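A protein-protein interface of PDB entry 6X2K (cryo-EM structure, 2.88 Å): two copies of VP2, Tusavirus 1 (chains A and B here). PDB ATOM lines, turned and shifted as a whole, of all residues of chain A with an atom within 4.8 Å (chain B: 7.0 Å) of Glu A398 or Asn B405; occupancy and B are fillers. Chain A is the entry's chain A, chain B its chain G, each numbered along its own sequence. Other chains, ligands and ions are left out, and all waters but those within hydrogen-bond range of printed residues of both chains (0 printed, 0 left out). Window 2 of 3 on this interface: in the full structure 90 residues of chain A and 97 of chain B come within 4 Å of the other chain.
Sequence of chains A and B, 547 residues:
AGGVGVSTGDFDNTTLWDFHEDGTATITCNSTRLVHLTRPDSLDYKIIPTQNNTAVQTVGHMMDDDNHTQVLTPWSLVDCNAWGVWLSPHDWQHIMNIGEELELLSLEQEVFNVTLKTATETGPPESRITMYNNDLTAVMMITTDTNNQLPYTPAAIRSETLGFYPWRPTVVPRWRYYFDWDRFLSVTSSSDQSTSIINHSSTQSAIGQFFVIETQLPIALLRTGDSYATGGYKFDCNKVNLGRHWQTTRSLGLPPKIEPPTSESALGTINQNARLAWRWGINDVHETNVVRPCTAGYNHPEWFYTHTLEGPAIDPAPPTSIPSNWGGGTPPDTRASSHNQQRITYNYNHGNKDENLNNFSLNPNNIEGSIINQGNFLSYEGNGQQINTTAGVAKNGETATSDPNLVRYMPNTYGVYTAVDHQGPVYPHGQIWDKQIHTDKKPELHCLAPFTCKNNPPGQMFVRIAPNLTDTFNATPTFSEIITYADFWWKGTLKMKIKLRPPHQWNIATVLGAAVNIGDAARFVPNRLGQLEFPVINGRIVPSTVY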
ATOM      1  N   PHE A 377     -11.679 -15.046 -21.408  1.00  0.00           N
ATOM      2  CA  PHE A 377     -12.070 -15.812 -20.238  1.00  0.00           C
ATOM      3  C   PHE A 377     -11.946 -14.936 -19.003  1.00  0.00           C
ATOM      4  O   PHE A 377     -11.200 -13.958 -18.980  1.00  0.00           O
ATOM      5  CB  PHE A 377     -11.238 -17.090 -20.095  1.00  0.00           C
ATOM      6  CG  PHE A 377      -9.782 -16.849 -19.898  1.00  0.00           C
ATOM      7  CD1 PHE A 377      -9.247 -16.795 -18.635  1.00  0.00           C
ATOM      8  CD2 PHE A 377      -8.950 -16.662 -20.975  1.00  0.00           C
ATOM      9  CE1 PHE A 377      -7.911 -16.576 -18.450  1.00  0.00           C
ATOM     10  CE2 PHE A 377      -7.618 -16.433 -20.793  1.00  0.00           C
ATOM     11  CZ  PHE A 377      -7.098 -16.392 -19.527  1.00  0.00           C
ATOM     12  N   LEU A 378     -12.696 -15.307 -17.973  1.00  0.00           N
ATOM     13  CA  LEU A 378     -12.787 -14.558 -16.731  1.00  0.00           C
ATOM     14  C   LEU A 378     -12.205 -15.390 -15.602  1.00  0.00           C
ATOM     15  O   LEU A 378     -12.372 -16.609 -15.576  1.00  0.00           O
ATOM     16  CB  LEU A 378     -14.238 -14.211 -16.416  1.00  0.00           C
ATOM     17  CG  LEU A 378     -14.550 -13.449 -15.131  1.00  0.00           C
ATOM     18  CD1 LEU A 378     -14.027 -12.037 -15.189  1.00  0.00           C
ATOM     19  CD2 LEU A 378     -16.032 -13.461 -14.863  1.00  0.00           C
ATOM     20  N   TYR A 380     -11.981 -15.304 -11.325  1.00  0.00           N
ATOM     21  CA  TYR A 380     -12.443 -14.605 -10.134  1.00  0.00           C
ATOM     22  C   TYR A 380     -11.288 -14.172  -9.252  1.00  0.00           C
ATOM     23  O   TYR A 380     -11.454 -13.291  -8.406  1.00  0.00           O
ATOM     24  CB  TYR A 380     -13.397 -15.472  -9.320  1.00  0.00           C
ATOM     25  CG  TYR A 380     -14.649 -15.911 -10.035  1.00  0.00           C
ATOM     26  CD1 TYR A 380     -15.156 -15.197 -11.096  1.00  0.00           C
ATOM     27  CD2 TYR A 380     -15.377 -16.981  -9.569  1.00  0.00           C
ATOM     28  CE1 TYR A 380     -16.308 -15.595 -11.723  1.00  0.00           C
ATOM     29  CE2 TYR A 380     -16.531 -17.376 -10.177  1.00  0.00           C
ATOM     30  CZ  TYR A 380     -16.995 -16.681 -11.252  1.00  0.00           C
ATOM     31  OH  TYR A 380     -18.157 -17.073 -11.861  1.00  0.00           O
ATOM     32  N   THR A 389     -14.501 -24.057 -14.257  1.00  0.00           N
ATOM     33  CA  THR A 389     -15.750 -23.442 -14.679  1.00  0.00           C
ATOM     34  C   THR A 389     -16.987 -24.230 -14.285  1.00  0.00           C
ATOM     35  O   THR A 389     -18.090 -23.835 -14.663  1.00  0.00           O
ATOM     36  CB  THR A 389     -15.760 -23.229 -16.192  1.00  0.00           C
ATOM     37  OG1 THR A 389     -15.590 -24.488 -16.846  1.00  0.00           O
ATOM     38  CG2 THR A 389     -14.647 -22.299 -16.600  1.00  0.00           C
ATOM     39  N   LYS A 395     -15.194 -22.736  -8.058  1.00  0.00           N
ATOM     40  CA  LYS A 395     -15.530 -22.081  -9.313  1.00  0.00           C
ATOM     41  C   LYS A 395     -14.694 -20.814  -9.291  1.00  0.00           C
ATOM     42  O   LYS A 395     -15.023 -19.869  -8.573  1.00  0.00           O
ATOM     43  CB  LYS A 395     -17.021 -21.784  -9.364  1.00  0.00           C
ATOM     44  CG  LYS A 395     -17.535 -21.030 -10.565  1.00  0.00           C
ATOM     45  CD  LYS A 395     -17.601 -21.869 -11.800  1.00  0.00           C
ATOM     46  CE  LYS A 395     -18.209 -21.063 -12.914  1.00  0.00           C
ATOM     47  NZ  LYS A 395     -19.594 -20.686 -12.565  1.00  0.00           N
ATOM     48  N   ASN A 396     -13.613 -20.789 -10.052  1.00  0.00           N
ATOM     49  CA  ASN A 396     -12.722 -19.643 -10.057  1.00  0.00           C
ATOM     50  C   ASN A 396     -12.855 -18.753 -11.281  1.00  0.00           C
ATOM     51  O   ASN A 396     -12.107 -17.779 -11.394  1.00  0.00           O
ATOM     52  CB  ASN A 396     -11.280 -20.102  -9.860  1.00  0.00           C
ATOM     53  CG  ASN A 396     -10.932 -21.278 -10.706  1.00  0.00           C
ATOM     54  OD1 ASN A 396     -11.513 -21.487 -11.764  1.00  0.00           O
ATOM     55  ND2 ASN A 396      -9.972 -22.063 -10.251  1.00  0.00           N
ATOM     56  N   GLY A 397     -13.770 -19.046 -12.196  1.00  0.00           N
ATOM     57  CA  GLY A 397     -13.947 -18.184 -13.344  1.00  0.00           C
ATOM     58  C   GLY A 397     -14.832 -18.836 -14.384  1.00  0.00           C
ATOM     59  O   GLY A 397     -15.475 -19.852 -14.127  1.00  0.00           O
ATOM     60  N   GLU A 398     -14.856 -18.220 -15.565  1.00  0.00           N
ATOM     61  CA  GLU A 398     -15.599 -18.744 -16.701  1.00  0.00           C
ATOM     62  C   GLU A 398     -14.874 -18.407 -17.991  1.00  0.00           C
ATOM     63  O   GLU A 398     -14.093 -17.458 -18.056  1.00  0.00           O
ATOM     64  CB  GLU A 398     -17.022 -18.198 -16.761  1.00  0.00           C
ATOM     65  CG  GLU A 398     -17.924 -18.713 -15.677  1.00  0.00           C
ATOM     66  CD  GLU A 398     -19.312 -18.175 -15.814  1.00  0.00           C
ATOM     67  OE1 GLU A 398     -19.499 -17.278 -16.656  1.00  0.00           O
ATOM     68  OE2 GLU A 398     -20.216 -18.643 -15.092  1.00  0.00           O
ATOM     69  N   THR A 399     -15.156 -19.193 -19.023  1.00  0.00           N
ATOM     70  CA  THR A 399     -14.520 -19.058 -20.321  1.00  0.00           C
ATOM     71  C   THR A 399     -15.574 -18.832 -21.392  1.00  0.00           C
ATOM     72  O   THR A 399     -16.759 -19.094 -21.189  1.00  0.00           O
ATOM     73  CB  THR A 399     -13.696 -20.298 -20.677  1.00  0.00           C
ATOM     74  OG1 THR A 399     -14.555 -21.438 -20.747  1.00  0.00           O
ATOM     75  CG2 THR A 399     -12.648 -20.555 -19.629  1.00  0.00           C
ATOM     76  N   ALA A 400     -15.123 -18.348 -22.549  1.00  0.00           N
ATOM     77  CA  ALA A 400     -16.040 -18.038 -23.638  1.00  0.00           C
ATOM     78  C   ALA A 400     -16.834 -19.249 -24.094  1.00  0.00           C
ATOM     79  O   ALA A 400     -17.886 -19.085 -24.716  1.00  0.00           O
ATOM     80  CB  ALA A 400     -15.276 -17.454 -24.820  1.00  0.00           C
ATOM     81  N   SER A 402     -17.762 -21.537 -21.745  1.00  0.00           N
ATOM     82  CA  SER A 402     -18.600 -21.852 -20.592  1.00  0.00           C
ATOM     83  C   SER A 402     -19.896 -21.052 -20.604  1.00  0.00           C
ATOM     84  O   SER A 402     -20.990 -21.625 -20.614  1.00  0.00           O
ATOM     85  CB  SER A 402     -17.819 -21.589 -19.308  1.00  0.00           C
ATOM     86  OG  SER A 402     -18.631 -21.795 -18.173  1.00  0.00           O
ATOM     87  N   ASP A 403     -19.793 -19.724 -20.621  1.00  0.00           N
ATOM     88  CA  ASP A 403     -20.943 -18.831 -20.751  1.00  0.00           C
ATOM     89  C   ASP A 403     -20.636 -17.849 -21.868  1.00  0.00           C
ATOM     90  O   ASP A 403     -20.094 -16.762 -21.629  1.00  0.00           O
ATOM     91  CB  ASP A 403     -21.256 -18.093 -19.453  1.00  0.00           C
ATOM     92  CG  ASP A 403     -21.950 -18.972 -18.431  1.00  0.00           C
ATOM     93  OD1 ASP A 403     -22.424 -20.066 -18.804  1.00  0.00           O
ATOM     94  OD2 ASP A 403     -22.038 -18.558 -17.257  1.00  0.00           O
ATOM     95  N   LEU A 406     -22.002 -14.124 -21.566  1.00  0.00           N
ATOM     96  CA  LEU A 406     -21.411 -13.217 -20.596  1.00  0.00           C
ATOM     97  C   LEU A 406     -20.016 -12.786 -21.019  1.00  0.00           C
ATOM     98  O   LEU A 406     -19.638 -11.624 -20.840  1.00  0.00           O
ATOM     99  CB  LEU A 406     -21.366 -13.892 -19.233  1.00  0.00           C
ATOM    100  CG  LEU A 406     -20.798 -13.035 -18.118  1.00  0.00           C
ATOM    101  CD1 LEU A 406     -21.756 -11.909 -17.792  1.00  0.00           C
ATOM    102  CD2 LEU A 406     -20.506 -13.889 -16.922  1.00  0.00           C
ATOM    103  N   VAL A 407     -19.244 -13.703 -21.588  1.00  0.00           N
ATOM    104  CA  VAL A 407     -17.845 -13.457 -21.902  1.00  0.00           C
ATOM    105  C   VAL A 407     -17.673 -13.094 -23.368  1.00  0.00           C
ATOM    106  O   VAL A 407     -17.161 -12.020 -23.689  1.00  0.00           O
ATOM    107  CB  VAL A 407     -16.976 -14.665 -21.529  1.00  0.00           C
ATOM    108  CG1 VAL A 407     -15.592 -14.451 -22.027  1.00  0.00           C
ATOM    109  CG2 VAL A 407     -16.952 -14.833 -20.036  1.00  0.00           C
ATOM    110  N   VAL B 187      -9.346 -21.770 -25.016  1.00  0.00           N
ATOM    111  CA  VAL B 187      -9.713 -21.763 -23.607  1.00  0.00           C
ATOM    112  C   VAL B 187     -10.221 -23.140 -23.217  1.00  0.00           C
ATOM    113  O   VAL B 187     -11.022 -23.749 -23.935  1.00  0.00           O
ATOM    114  CB  VAL B 187     -10.761 -20.678 -23.312  1.00  0.00           C
ATOM    115  CG1 VAL B 187     -10.164 -19.314 -23.506  1.00  0.00           C
ATOM    116  CG2 VAL B 187     -11.954 -20.834 -24.212  1.00  0.00           C
ATOM    117  N   PHE B 304     -10.452  -9.934 -16.143  1.00  0.00           N
ATOM    118  CA  PHE B 304     -10.861 -10.397 -17.453  1.00  0.00           C
ATOM    119  C   PHE B 304      -9.705 -10.405 -18.432  1.00  0.00           C
ATOM    120  O   PHE B 304      -9.119  -9.372 -18.712  1.00  0.00           O
ATOM    121  CB  PHE B 304     -11.985  -9.503 -17.969  1.00  0.00           C
ATOM    122  CG  PHE B 304     -12.575  -9.955 -19.265  1.00  0.00           C
ATOM    123  CD1 PHE B 304     -13.646 -10.821 -19.284  1.00  0.00           C
ATOM    124  CD2 PHE B 304     -12.064  -9.504 -20.463  1.00  0.00           C
ATOM    125  CE1 PHE B 304     -14.192 -11.238 -20.477  1.00  0.00           C
ATOM    126  CE2 PHE B 304     -12.605  -9.915 -21.658  1.00  0.00           C
ATOM    127  CZ  PHE B 304     -13.670 -10.785 -21.665  1.00  0.00           C
ATOM    128  N   ALA B 400     -25.212  -9.053  -5.760  1.00  0.00           N
ATOM    129  CA  ALA B 400     -23.939  -9.700  -6.051  1.00  0.00           C
ATOM    130  C   ALA B 400     -23.877 -11.126  -5.534  1.00  0.00           C
ATOM    131  O   ALA B 400     -23.055 -11.910  -6.013  1.00  0.00           O
ATOM    132  CB  ALA B 400     -22.791  -8.892  -5.458  1.00  0.00           C
ATOM    133  N   SER B 402     -26.735 -12.982  -5.605  1.00  0.00           N
ATOM    134  CA  SER B 402     -27.733 -13.681  -6.408  1.00  0.00           C
ATOM    135  C   SER B 402     -27.147 -14.179  -7.723  1.00  0.00           C
ATOM    136  O   SER B 402     -27.165 -15.381  -8.006  1.00  0.00           O
ATOM    137  CB  SER B 402     -28.918 -12.756  -6.665  1.00  0.00           C
ATOM    138  OG  SER B 402     -29.860 -13.370  -7.517  1.00  0.00           O
ATOM    139  N   ASP B 403     -26.607 -13.271  -8.533  1.00  0.00           N
ATOM    140  CA  ASP B 403     -25.905 -13.612  -9.769  1.00  0.00           C
ATOM    141  C   ASP B 403     -24.564 -12.900  -9.747  1.00  0.00           C
ATOM    142  O   ASP B 403     -24.435 -11.772 -10.241  1.00  0.00           O
ATOM    143  CB  ASP B 403     -26.700 -13.231 -11.014  1.00  0.00           C
ATOM    144  CG  ASP B 403     -27.840 -14.188 -11.298  1.00  0.00           C
ATOM    145  OD1 ASP B 403     -27.866 -15.284 -10.700  1.00  0.00           O
ATOM    146  OD2 ASP B 403     -28.700 -13.851 -12.137  1.00  0.00           O
ATOM    147  N   PRO B 404     -23.541 -13.530  -9.179  1.00  0.00           N
ATOM    148  CA  PRO B 404     -22.254 -12.841  -9.042  1.00  0.00           C
ATOM    149  C   PRO B 404     -21.618 -12.498 -10.368  1.00  0.00           C
ATOM    150  O   PRO B 404     -20.970 -11.456 -10.482  1.00  0.00           O
ATOM    151  CB  PRO B 404     -21.418 -13.851  -8.253  1.00  0.00           C
ATOM    152  CG  PRO B 404     -22.416 -14.677  -7.536  1.00  0.00           C
ATOM    153  CD  PRO B 404     -23.547 -14.822  -8.485  1.00  0.00           C
ATOM    154  N   ASN B 405     -21.777 -13.356 -11.375  1.00  0.00           N
ATOM    155  CA  ASN B 405     -21.205 -13.081 -12.688  1.00  0.00           C
ATOM    156  C   ASN B 405     -21.734 -11.777 -13.254  1.00  0.00           C
ATOM    157  O   ASN B 405     -20.974 -10.946 -13.757  1.00  0.00           O
ATOM    158  CB  ASN B 405     -21.515 -14.224 -13.646  1.00  0.00           C
ATOM    159  CG  ASN B 405     -20.678 -15.439 -13.392  1.00  0.00           C
ATOM    160  OD1 ASN B 405     -19.607 -15.356 -12.804  1.00  0.00           O
ATOM    161  ND2 ASN B 405     -21.148 -16.584 -13.856  1.00  0.00           N
ATOM    162  N   LEU B 406     -23.045 -11.580 -13.180  1.00  0.00           N
ATOM    163  CA  LEU B 406     -23.650 -10.437 -13.843  1.00  0.00           C
ATOM    164  C   LEU B 406     -23.362  -9.146 -13.094  1.00  0.00           C
ATOM    165  O   LEU B 406     -23.116  -8.105 -13.712  1.00  0.00           O
ATOM    166  CB  LEU B 406     -25.151 -10.656 -13.961  1.00  0.00           C
ATOM    167  CG  LEU B 406     -25.903  -9.544 -14.668  1.00  0.00           C
ATOM    168  CD1 LEU B 406     -25.549  -9.535 -16.140  1.00  0.00           C
ATOM    169  CD2 LEU B 406     -27.374  -9.707 -14.444  1.00  0.00           C
ATOM    170  N   VAL B 407     -23.378  -9.197 -11.769  1.00  0.00           N
ATOM    171  CA  VAL B 407     -23.263  -8.004 -10.943  1.00  0.00           C
ATOM    172  C   VAL B 407     -21.839  -7.826 -10.441  1.00  0.00           C
ATOM    173  O   VAL B 407     -21.211  -6.799 -10.700  1.00  0.00           O
ATOM    174  CB  VAL B 407     -24.257  -8.046  -9.775  1.00  0.00           C
ATOM    175  CG1 VAL B 407     -23.989  -6.909  -8.856  1.00  0.00           C
ATOM    176  CG2 VAL B 407     -25.662  -7.948 -10.299  1.00  0.00           C
ATOM    177  N   ARG B 408     -21.331  -8.799  -9.688  1.00  0.00           N
ATOM    178  CA  ARG B 408     -20.029  -8.635  -9.057  1.00  0.00           C
ATOM    179  C   ARG B 408     -18.897  -8.645 -10.077  1.00  0.00           C
ATOM    180  O   ARG B 408     -18.076  -7.728 -10.114  1.00  0.00           O
ATOM    181  CB  ARG B 408     -19.820  -9.731  -8.016  1.00  0.00           C
ATOM    182  CG  ARG B 408     -18.513  -9.614  -7.271  1.00  0.00           C
ATOM    183  CD  ARG B 408     -18.394 -10.663  -6.205  1.00  0.00           C
ATOM    184  NE  ARG B 408     -17.151 -10.523  -5.461  1.00  0.00           N
ATOM    185  CZ  ARG B 408     -16.865 -11.196  -4.356  1.00  0.00           C
ATOM    186  NH1 ARG B 408     -17.734 -12.056  -3.862  1.00  0.00           N
ATOM    187  NH2 ARG B 408     -15.711 -11.005  -3.748  1.00  0.00           N
ATOM    188  N   TYR B 409     -18.826  -9.682 -10.901  1.00  0.00           N
ATOM    189  CA  TYR B 409     -17.615  -9.955 -11.669  1.00  0.00           C
ATOM    190  C   TYR B 409     -17.532  -9.177 -12.980  1.00  0.00           C
ATOM    191  O   TYR B 409     -16.451  -8.705 -13.340  1.00  0.00           O
ATOM    192  CB  TYR B 409     -17.503 -11.455 -11.900  1.00  0.00           C
ATOM    193  CG  TYR B 409     -17.238 -12.203 -10.619  1.00  0.00           C
ATOM    194  CD1 TYR B 409     -16.215 -11.815  -9.774  1.00  0.00           C
ATOM    195  CD2 TYR B 409     -18.053 -13.236 -10.217  1.00  0.00           C
ATOM    196  CE1 TYR B 409     -15.977 -12.476  -8.602  1.00  0.00           C
ATOM    197  CE2 TYR B 409     -17.824 -13.899  -9.040  1.00  0.00           C
ATOM    198  CZ  TYR B 409     -16.787 -13.512  -8.236  1.00  0.00           C
ATOM    199  OH  TYR B 409     -16.560 -14.177  -7.060  1.00  0.00           O
ATOM    200  N   MET B 410     -18.637  -9.012 -13.714  1.00  0.00           N
ATOM    201  CA  MET B 410     -18.581  -8.406 -15.049  1.00  0.00           C
ATOM    202  C   MET B 410     -19.532  -7.221 -15.230  1.00  0.00           C
ATOM    203  O   MET B 410     -20.291  -7.178 -16.195  1.00  0.00           O
ATOM    204  CB  MET B 410     -18.925  -9.474 -16.083  1.00  0.00           C
ATOM    205  CG  MET B 410     -17.952 -10.603 -16.264  1.00  0.00           C
ATOM    206  SD  MET B 410     -16.467 -10.127 -17.133  1.00  0.00           S
ATOM    207  CE  MET B 410     -17.154  -9.846 -18.751  1.00  0.00           C
ATOM    208  N   PRO B 411     -19.502  -6.224 -14.347  1.00  0.00           N
ATOM    209  CA  PRO B 411     -20.117  -4.942 -14.689  1.00  0.00           C
ATOM    210  C   PRO B 411     -19.146  -4.026 -15.408  1.00  0.00           C
ATOM    211  O   PRO B 411     -17.936  -4.092 -15.215  1.00  0.00           O
ATOM    212  CB  PRO B 411     -20.508  -4.376 -13.321  1.00  0.00           C
ATOM    213  CG  PRO B 411     -19.480  -4.878 -12.447  1.00  0.00           C
ATOM    214  CD  PRO B 411     -19.059  -6.219 -12.946  1.00  0.00           C
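OD1 of Asn B405 lies within hydrogen-bond range of OH of Tyr A380, 2.4 Å away. The side-chain carboxylate of Glu A398 lies within hydrogen-bond range of the side-chain amide nitrogen of Asn B405 (2.6 Å).
O of Glu A398 is in hydrogen-bond range of N of Leu A378 (2.6 Å). The backbone NH (N) of Tyr A380 lies within hydrogen-bond range of the backbone carbonyl oxygen (O) of Asn A396. NZ of Lys A395 is in salt-bridge range of OE2 of Glu A398, at 3.3 Å. The side-chain hydroxyl (OG1) of Thr A399 lies within hydrogen-bond range of the backbone NH (N) of Ser A402 (3.4 Å). N of Tyr B409 sits at hydrogen-bond distance from O of Pro B404. O of Asn B405 sits at hydrogen-bond distance from N of Met B410 (3.0 Å).
Among the printed residues, merely in contact across the chains: Phe A377 with Val B187, Phe A377 with Phe B304, Leu A378 with Tyr B409, Leu A378 with Met B410, Tyr A380 with Tyr B409, Thr A399 with Val B187, Leu A406 with Asn B405, Leu A406 with Met B410 and Val A407 with Phe B304.
Of the printed residues of chain B, Leu A378 touches Tyr B409 (3.9 Å) and Met B410 (3.7 Å). Printed residues of chain B within 4 Å of Glu A398: Asn B405. Printed residues of chain B within 4 Å of Val A407: Phe B304. Of the printed residues of chain A, Phe B304 touches Phe A377 (3.9 Å) and Val A407 (3.8 Å). Pro B404 touches none of the printed residues of chain A. Of chain A, only Tyr A380 (2.4 Å), Glu A398 (2.6 Å) and Leu A406 (3.4 Å) come within 4 Å of Asn B405. Val B407 touches none of the printed residues of chain A. Of the printed residues of chain A, Tyr B409 touches Leu A378 and Tyr A380. Of the printed residues of chain A, Met B410 touches Leu A378 and Leu A406. The nearest residue of chain B that does not touch Glu A398 is Phe B304 (6.7 Å).
Of the 14 printed residues of chain A, 7 touch a printed residue of chain B. Along chain A the printed residues that touch a printed residue of chain B span positions 377 to 407. Among the printed residues, 11 pairs touch across the chains. Among the printed residues, no Asp or Glu carboxylate lies within 4 Å of a Lys or Arg side-chain nitrogen of the other chain.
Positions printed for both chains: 400, 402, 403, 406 and 407. Of the 11 pairs that touch across the chains among the printed residues, none has its exchanged pair printed and touching as well.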
